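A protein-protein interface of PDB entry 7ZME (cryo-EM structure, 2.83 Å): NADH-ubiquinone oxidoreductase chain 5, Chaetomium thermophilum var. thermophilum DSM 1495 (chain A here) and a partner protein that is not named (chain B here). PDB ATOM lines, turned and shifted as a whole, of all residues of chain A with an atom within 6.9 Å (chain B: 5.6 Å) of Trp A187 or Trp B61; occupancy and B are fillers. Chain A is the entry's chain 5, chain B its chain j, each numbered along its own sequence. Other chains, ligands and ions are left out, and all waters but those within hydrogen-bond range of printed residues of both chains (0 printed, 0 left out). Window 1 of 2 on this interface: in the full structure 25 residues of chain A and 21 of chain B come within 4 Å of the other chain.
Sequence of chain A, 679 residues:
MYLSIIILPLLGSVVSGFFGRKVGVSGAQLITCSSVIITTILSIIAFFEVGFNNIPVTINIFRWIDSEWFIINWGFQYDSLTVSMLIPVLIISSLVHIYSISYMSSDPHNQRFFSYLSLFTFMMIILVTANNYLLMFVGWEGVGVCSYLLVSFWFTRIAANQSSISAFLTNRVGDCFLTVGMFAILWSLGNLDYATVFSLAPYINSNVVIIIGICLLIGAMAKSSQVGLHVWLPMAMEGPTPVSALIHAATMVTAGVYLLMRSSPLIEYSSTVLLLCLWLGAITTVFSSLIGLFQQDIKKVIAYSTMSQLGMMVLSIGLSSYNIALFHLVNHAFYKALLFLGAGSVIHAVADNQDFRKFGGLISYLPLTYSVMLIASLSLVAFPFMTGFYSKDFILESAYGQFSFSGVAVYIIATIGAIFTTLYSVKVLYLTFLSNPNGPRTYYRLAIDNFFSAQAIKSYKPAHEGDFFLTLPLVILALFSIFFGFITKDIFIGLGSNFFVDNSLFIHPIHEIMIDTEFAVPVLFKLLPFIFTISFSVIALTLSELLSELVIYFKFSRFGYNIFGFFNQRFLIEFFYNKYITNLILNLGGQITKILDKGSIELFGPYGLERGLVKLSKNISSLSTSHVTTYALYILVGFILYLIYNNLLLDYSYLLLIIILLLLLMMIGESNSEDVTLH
The indole nitrogen (NE1) of Trp A187 is in hydrogen-bond range of the side-chain carboxylate (OD1) of Asp B62 (2.9 Å).
O of Arg B64 lies close to O of Ser A188, 2.7 Å away.
The guanidinium group of Arg B64 sits at hydrogen-bond distance from the backbone carbonyl oxygen of Trp A187 (2.9 Å).
The guanidinium group (NH2) of Arg B64 sits at hydrogen-bond distance from the backbone carbonyl oxygen (O) of Leu A186, at 3.4 Å.
The backbone NH of Asp B62 is in hydrogen-bond range of the backbone carbonyl oxygen of Ile B72, 3.0 Å away.
The backbone carbonyl oxygen (O) of Ala A184 sits at hydrogen-bond distance from the side-chain hydroxyl (OG) of Ser A188, at 2.9 Å.
The backbone NH of Arg B64 lies within hydrogen-bond range of the side-chain carboxylate of Asp B62, 3.5 Å away.
CD2 of Leu B63 touches O of Ala A184, at 3.8 Å.
Trp A187 touches Trp B61.
NE1 of Trp A187 touches N of Leu B63, at 3.5 Å.
O of Leu B63 touches CA of Ser A188 (3.2 Å).
Ser A188 touches Ala B65.
Leu A189 touches Arg B64.
CA of Gly A190 touches NH1 of Arg B64 (3.4 Å).
Of chain B, only Trp B61 (3.8 Å), Asp B62 (2.9 Å), Leu B63 (3.5 Å) and Arg B64 (2.9 Å) come within 4 Å of Trp A187.
Trp B61 touches just one residue of chain A: Trp A187.
Printed residues of chain A within 4 Å of Asp B62: Trp A187 (2.9 Å).
Printed residues of chain B within 4 Å of Leu A189: Arg B64.
Printed residues of chain B within 4 Å of Leu A186: Arg B64.
Of the printed residues of chain A, Arg B64 touches Leu A186, Trp A187, Ser A188, Leu A189 and Gly A190.
Printed residues of chain B within 4 Å of Gly A190: Arg B64 (3.4 Å).
Ser B73 touches none of the printed residues of chain A.
The nearest residue of chain B that does not touch Trp A187 is Ala B65 (4.9 Å).
The nearest printed residue of chain A that does not touch Trp B61 is Ser A188 (10.1 Å).
The nearest printed residue of chain A that does not touch Leu B63 is Leu A189 (5.3 Å).
Of the 11 printed residues of chain A, 6 touch a printed residue of chain B.
Hydrophobic or aromatic side chains of chain A that line the printed part of chain B: Trp A187.
Among the printed residues, no Asp or Glu carboxylate lies within 4 Å of a Lys or Arg side-chain nitrogen of the other chain.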
ATOM      1  N   PHE A  70      30.119 -18.795   4.357  1.00  0.00           N
ATOM      2  CA  PHE A  70      29.499 -18.616   3.052  1.00  0.00           C
ATOM      3  C   PHE A  70      30.568 -18.260   2.031  1.00  0.00           C
ATOM      4  O   PHE A  70      31.310 -17.291   2.210  1.00  0.00           O
ATOM      5  CB  PHE A  70      28.427 -17.530   3.113  1.00  0.00           C
ATOM      6  CG  PHE A  70      27.447 -17.700   4.241  1.00  0.00           C
ATOM      7  CD1 PHE A  70      27.213 -18.945   4.803  1.00  0.00           C
ATOM      8  CD2 PHE A  70      26.756 -16.611   4.744  1.00  0.00           C
ATOM      9  CE1 PHE A  70      26.321 -19.098   5.838  1.00  0.00           C
ATOM     10  CE2 PHE A  70      25.859 -16.764   5.779  1.00  0.00           C
ATOM     11  CZ  PHE A  70      25.643 -18.007   6.323  1.00  0.00           C
ATOM     12  N   MET A 182      16.499 -17.596   0.660  1.00  0.00           N
ATOM     13  CA  MET A 182      17.937 -17.830   0.632  1.00  0.00           C
ATOM     14  C   MET A 182      18.553 -17.672   2.014  1.00  0.00           C
ATOM     15  O   MET A 182      19.521 -18.366   2.339  1.00  0.00           O
ATOM     16  CB  MET A 182      18.599 -16.884  -0.366  1.00  0.00           C
ATOM     17  CG  MET A 182      18.009 -16.960  -1.759  1.00  0.00           C
ATOM     18  SD  MET A 182      19.005 -16.117  -2.998  1.00  0.00           S
ATOM     19  CE  MET A 182      18.299 -14.475  -2.949  1.00  0.00           C
ATOM     20  N   PHE A 183      18.010 -16.771   2.835  1.00  0.00           N
ATOM     21  CA  PHE A 183      18.464 -16.664   4.219  1.00  0.00           C
ATOM     22  C   PHE A 183      18.219 -17.961   4.974  1.00  0.00           C
ATOM     23  O   PHE A 183      19.062 -18.399   5.762  1.00  0.00           O
ATOM     24  CB  PHE A 183      17.752 -15.515   4.926  1.00  0.00           C
ATOM     25  CG  PHE A 183      18.219 -14.154   4.519  1.00  0.00           C
ATOM     26  CD1 PHE A 183      19.450 -13.968   3.931  1.00  0.00           C
ATOM     27  CD2 PHE A 183      17.416 -13.050   4.739  1.00  0.00           C
ATOM     28  CE1 PHE A 183      19.868 -12.708   3.569  1.00  0.00           C
ATOM     29  CE2 PHE A 183      17.827 -11.793   4.369  1.00  0.00           C
ATOM     30  CZ  PHE A 183      19.055 -11.622   3.783  1.00  0.00           C
ATOM     31  N   ALA A 184      17.056 -18.583   4.753  1.00  0.00           N
ATOM     32  CA  ALA A 184      16.761 -19.872   5.367  1.00  0.00           C
ATOM     33  C   ALA A 184      17.688 -20.964   4.860  1.00  0.00           C
ATOM     34  O   ALA A 184      18.022 -21.886   5.609  1.00  0.00           O
ATOM     35  CB  ALA A 184      15.307 -20.255   5.108  1.00  0.00           C
ATOM     36  N   ILE A 185      18.102 -20.889   3.594  1.00  0.00           N
ATOM     37  CA  ILE A 185      19.032 -21.874   3.053  1.00  0.00           C
ATOM     38  C   ILE A 185      20.416 -21.695   3.663  1.00  0.00           C
ATOM     39  O   ILE A 185      21.078 -22.672   4.028  1.00  0.00           O
ATOM     40  CB  ILE A 185      19.067 -21.774   1.516  1.00  0.00           C
ATOM     41  CG1 ILE A 185      17.766 -22.301   0.917  1.00  0.00           C
ATOM     42  CG2 ILE A 185      20.251 -22.536   0.945  1.00  0.00           C
ATOM     43  CD1 ILE A 185      17.670 -22.100  -0.570  1.00  0.00           C
ATOM     44  N   LEU A 186      20.876 -20.447   3.786  1.00  0.00           N
ATOM     45  CA  LEU A 186      22.170 -20.185   4.409  1.00  0.00           C
ATOM     46  C   LEU A 186      22.168 -20.586   5.876  1.00  0.00           C
ATOM     47  O   LEU A 186      23.167 -21.099   6.388  1.00  0.00           O
ATOM     48  CB  LEU A 186      22.538 -18.708   4.276  1.00  0.00           C
ATOM     49  CG  LEU A 186      23.169 -18.218   2.979  1.00  0.00           C
ATOM     50  CD1 LEU A 186      23.475 -16.734   3.085  1.00  0.00           C
ATOM     51  CD2 LEU A 186      24.419 -19.009   2.646  1.00  0.00           C
ATOM     52  N   TRP A 187      21.058 -20.336   6.573  1.00  0.00           N
ATOM     53  CA  TRP A 187      20.973 -20.694   7.982  1.00  0.00           C
ATOM     54  C   TRP A 187      21.117 -22.196   8.175  1.00  0.00           C
ATOM     55  O   TRP A 187      21.921 -22.654   8.992  1.00  0.00           O
ATOM     56  CB  TRP A 187      19.650 -20.203   8.569  1.00  0.00           C
ATOM     57  CG  TRP A 187      19.621 -20.179  10.071  1.00  0.00           C
ATOM     58  CD1 TRP A 187      20.564 -20.678  10.917  1.00  0.00           C
ATOM     59  CD2 TRP A 187      18.590 -19.638  10.898  1.00  0.00           C
ATOM     60  NE1 TRP A 187      20.188 -20.477  12.217  1.00  0.00           N
ATOM     61  CE2 TRP A 187      18.976 -19.841  12.233  1.00  0.00           C
ATOM     62  CE3 TRP A 187      17.376 -18.999  10.640  1.00  0.00           C
ATOM     63  CZ2 TRP A 187      18.195 -19.427  13.306  1.00  0.00           C
ATOM     64  CZ3 TRP A 187      16.604 -18.591  11.705  1.00  0.00           C
ATOM     65  CH2 TRP A 187      17.015 -18.805  13.020  1.00  0.00           C
ATOM     66  N   SER A 188      20.360 -22.980   7.415  1.00  0.00           N
ATOM     67  CA  SER A 188      20.300 -24.414   7.643  1.00  0.00           C
ATOM     68  C   SER A 188      21.384 -25.204   6.920  1.00  0.00           C
ATOM     69  O   SER A 188      21.570 -26.383   7.232  1.00  0.00           O
ATOM     70  CB  SER A 188      18.923 -24.951   7.246  1.00  0.00           C
ATOM     71  OG  SER A 188      18.662 -24.726   5.878  1.00  0.00           O
ATOM     72  N   LEU A 189      22.103 -24.610   5.971  1.00  0.00           N
ATOM     73  CA  LEU A 189      23.121 -25.351   5.238  1.00  0.00           C
ATOM     74  C   LEU A 189      24.500 -24.716   5.247  1.00  0.00           C
ATOM     75  O   LEU A 189      25.470 -25.405   4.910  1.00  0.00           O
ATOM     76  CB  LEU A 189      22.704 -25.564   3.774  1.00  0.00           C
ATOM     77  CG  LEU A 189      21.764 -26.728   3.436  1.00  0.00           C
ATOM     78  CD1 LEU A 189      22.422 -28.060   3.753  1.00  0.00           C
ATOM     79  CD2 LEU A 189      20.410 -26.608   4.100  1.00  0.00           C
ATOM     80  N   GLY A 190      24.632 -23.442   5.600  1.00  0.00           N
ATOM     81  CA  GLY A 190      25.921 -22.792   5.566  1.00  0.00           C
ATOM     82  C   GLY A 190      26.397 -22.410   4.185  1.00  0.00           C
ATOM     83  O   GLY A 190      27.516 -21.903   4.050  1.00  0.00           O
ATOM     84  N   ASN A 191      25.591 -22.649   3.159  1.00  0.00           N
ATOM     85  CA  ASN A 191      25.895 -22.234   1.799  1.00  0.00           C
ATOM     86  C   ASN A 191      24.621 -22.343   0.981  1.00  0.00           C
ATOM     87  O   ASN A 191      23.606 -22.872   1.438  1.00  0.00           O
ATOM     88  CB  ASN A 191      27.010 -23.072   1.172  1.00  0.00           C
ATOM     89  CG  ASN A 191      27.952 -22.241   0.336  1.00  0.00           C
ATOM     90  OD1 ASN A 191      28.351 -21.151   0.734  1.00  0.00           O
ATOM     91  ND2 ASN A 191      28.302 -22.746  -0.835  1.00  0.00           N
ATOM     92  N   THR B  57      10.193 -14.860  21.318  1.00  0.00           N
ATOM     93  CA  THR B  57      10.720 -15.745  20.289  1.00  0.00           C
ATOM     94  C   THR B  57      12.242 -15.761  20.265  1.00  0.00           C
ATOM     95  O   THR B  57      12.828 -16.210  19.274  1.00  0.00           O
ATOM     96  CB  THR B  57      10.188 -15.347  18.907  1.00  0.00           C
ATOM     97  OG1 THR B  57      10.514 -13.979  18.642  1.00  0.00           O
ATOM     98  CG2 THR B  57       8.682 -15.519  18.846  1.00  0.00           C
ATOM     99  N   GLY B  59      15.748 -17.104  20.898  1.00  0.00           N
ATOM    100  CA  GLY B  59      16.268 -18.428  21.141  1.00  0.00           C
ATOM    101  C   GLY B  59      15.304 -19.549  20.831  1.00  0.00           C
ATOM    102  O   GLY B  59      15.648 -20.715  21.047  1.00  0.00           O
ATOM    103  N   LEU B  60      14.110 -19.233  20.331  1.00  0.00           N
ATOM    104  CA  LEU B  60      13.088 -20.251  20.125  1.00  0.00           C
ATOM    105  C   LEU B  60      13.463 -21.209  19.003  1.00  0.00           C
ATOM    106  O   LEU B  60      13.220 -22.415  19.107  1.00  0.00           O
ATOM    107  CB  LEU B  60      11.745 -19.585  19.832  1.00  0.00           C
ATOM    108  CG  LEU B  60      10.509 -20.469  19.675  1.00  0.00           C
ATOM    109  CD1 LEU B  60      10.424 -21.507  20.783  1.00  0.00           C
ATOM    110  CD2 LEU B  60       9.271 -19.602  19.654  1.00  0.00           C
ATOM    111  N   TRP B  61      14.052 -20.698  17.927  1.00  0.00           N
ATOM    112  CA  TRP B  61      14.272 -21.480  16.724  1.00  0.00           C
ATOM    113  C   TRP B  61      15.730 -21.425  16.297  1.00  0.00           C
ATOM    114  O   TRP B  61      16.429 -20.436  16.532  1.00  0.00           O
ATOM    115  CB  TRP B  61      13.399 -20.978  15.580  1.00  0.00           C
ATOM    116  CG  TRP B  61      11.946 -21.109  15.837  1.00  0.00           C
ATOM    117  CD1 TRP B  61      11.274 -22.240  16.180  1.00  0.00           C
ATOM    118  CD2 TRP B  61      10.975 -20.064  15.777  1.00  0.00           C
ATOM    119  NE1 TRP B  61       9.940 -21.966  16.332  1.00  0.00           N
ATOM    120  CE2 TRP B  61       9.731 -20.635  16.089  1.00  0.00           C
ATOM    121  CE3 TRP B  61      11.037 -18.700  15.479  1.00  0.00           C
ATOM    122  CZ2 TRP B  61       8.558 -19.894  16.114  1.00  0.00           C
ATOM    123  CZ3 TRP B  61       9.877 -17.967  15.507  1.00  0.00           C
ATOM    124  CH2 TRP B  61       8.651 -18.563  15.824  1.00  0.00           C
ATOM    125  N   ASP B  62      16.175 -22.501  15.657  1.00  0.00           N
ATOM    126  CA  ASP B  62      17.501 -22.569  15.062  1.00  0.00           C
ATOM    127  C   ASP B  62      17.469 -23.582  13.933  1.00  0.00           C
ATOM    128  O   ASP B  62      16.963 -24.693  14.106  1.00  0.00           O
ATOM    129  CB  ASP B  62      18.559 -22.951  16.095  1.00  0.00           C
ATOM    130  CG  ASP B  62      19.963 -22.913  15.534  1.00  0.00           C
ATOM    131  OD1 ASP B  62      20.227 -22.058  14.665  1.00  0.00           O
ATOM    132  OD2 ASP B  62      20.803 -23.730  15.965  1.00  0.00           O
ATOM    133  N   LEU B  63      18.000 -23.192  12.780  1.00  0.00           N
ATOM    134  CA  LEU B  63      17.958 -24.014  11.583  1.00  0.00           C
ATOM    135  C   LEU B  63      19.278 -24.704  11.292  1.00  0.00           C
ATOM    136  O   LEU B  63      19.315 -25.575  10.421  1.00  0.00           O
ATOM    137  CB  LEU B  63      17.572 -23.153  10.375  1.00  0.00           C
ATOM    138  CG  LEU B  63      16.135 -23.159   9.868  1.00  0.00           C
ATOM    139  CD1 LEU B  63      15.183 -22.826  10.993  1.00  0.00           C
ATOM    140  CD2 LEU B  63      15.988 -22.153   8.756  1.00  0.00           C
ATOM    141  N   ARG B  64      20.330 -24.379  12.051  1.00  0.00           N
ATOM    142  CA  ARG B  64      21.715 -24.466  11.597  1.00  0.00           C
ATOM    143  C   ARG B  64      22.024 -25.723  10.796  1.00  0.00           C
ATOM    144  O   ARG B  64      22.477 -25.644   9.649  1.00  0.00           O
ATOM    145  CB  ARG B  64      22.660 -24.375  12.795  1.00  0.00           C
ATOM    146  CG  ARG B  64      24.120 -24.377  12.386  1.00  0.00           C
ATOM    147  CD  ARG B  64      24.475 -23.040  11.775  1.00  0.00           C
ATOM    148  NE  ARG B  64      25.560 -23.125  10.805  1.00  0.00           N
ATOM    149  CZ  ARG B  64      25.609 -22.418   9.683  1.00  0.00           C
ATOM    150  NH1 ARG B  64      26.634 -22.551   8.860  1.00  0.00           N
ATOM    151  NH2 ARG B  64      24.631 -21.577   9.385  1.00  0.00           N
ATOM    152  N   ALA B  65      21.832 -26.890  11.395  1.00  0.00           N
ATOM    153  CA  ALA B  65      22.107 -28.146  10.713  1.00  0.00           C
ATOM    154  C   ALA B  65      21.045 -29.181  11.047  1.00  0.00           C
ATOM    155  O   ALA B  65      21.345 -30.365  11.228  1.00  0.00           O
ATOM    156  CB  ALA B  65      23.501 -28.664  11.061  1.00  0.00           C
ATOM    157  N   ILE B  72      13.181 -27.689  14.736  1.00  0.00           N
ATOM    158  CA  ILE B  72      13.562 -26.284  14.644  1.00  0.00           C
ATOM    159  C   ILE B  72      13.580 -25.654  16.027  1.00  0.00           C
ATOM    160  O   ILE B  72      14.474 -24.867  16.359  1.00  0.00           O
ATOM    161  CB  ILE B  72      12.608 -25.533  13.699  1.00  0.00           C
ATOM    162  CG1 ILE B  72      12.593 -26.188  12.317  1.00  0.00           C
ATOM    163  CG2 ILE B  72      13.001 -24.075  13.599  1.00  0.00           C
ATOM    164  CD1 ILE B  72      11.668 -25.511  11.347  1.00  0.00           C
ATOM    165  N   SER B  73      12.596 -25.993  16.853  1.00  0.00           N
ATOM    166  CA  SER B  73      12.496 -25.419  18.185  1.00  0.00           C
ATOM    167  C   SER B  73      13.647 -25.881  19.064  1.00  0.00           C
ATOM    168  O   SER B  73      14.091 -27.028  18.988  1.00  0.00           O
ATOM    169  CB  SER B  73      11.164 -25.804  18.823  1.00  0.00           C
ATOM    170  OG  SER B  73      10.858 -24.959  19.914  1.00  0.00           O
ATOM    171  N   GLU B  74      14.144 -24.964  19.890  1.00  0.00           N
ATOM    172  CA  GLU B  74      15.107 -25.289  20.928  1.00  0.00           C
ATOM    173  C   GLU B  74      14.622 -24.920  22.318  1.00  0.00           C
ATOM    174  O   GLU B  74      15.227 -25.353  23.304  1.00  0.00           O
ATOM    175  CB  GLU B  74      16.449 -24.598  20.662  1.00  0.00           C
ATOM    176  CG  GLU B  74      17.170 -25.115  19.442  1.00  0.00           C
ATOM    177  CD  GLU B  74      18.478 -24.410  19.200  1.00  0.00           C
ATOM    178  OE1 GLU B  74      18.763 -23.424  19.913  1.00  0.00           O
ATOM    179  OE2 GLU B  74      19.252 -24.885  18.343  1.00  0.00           O
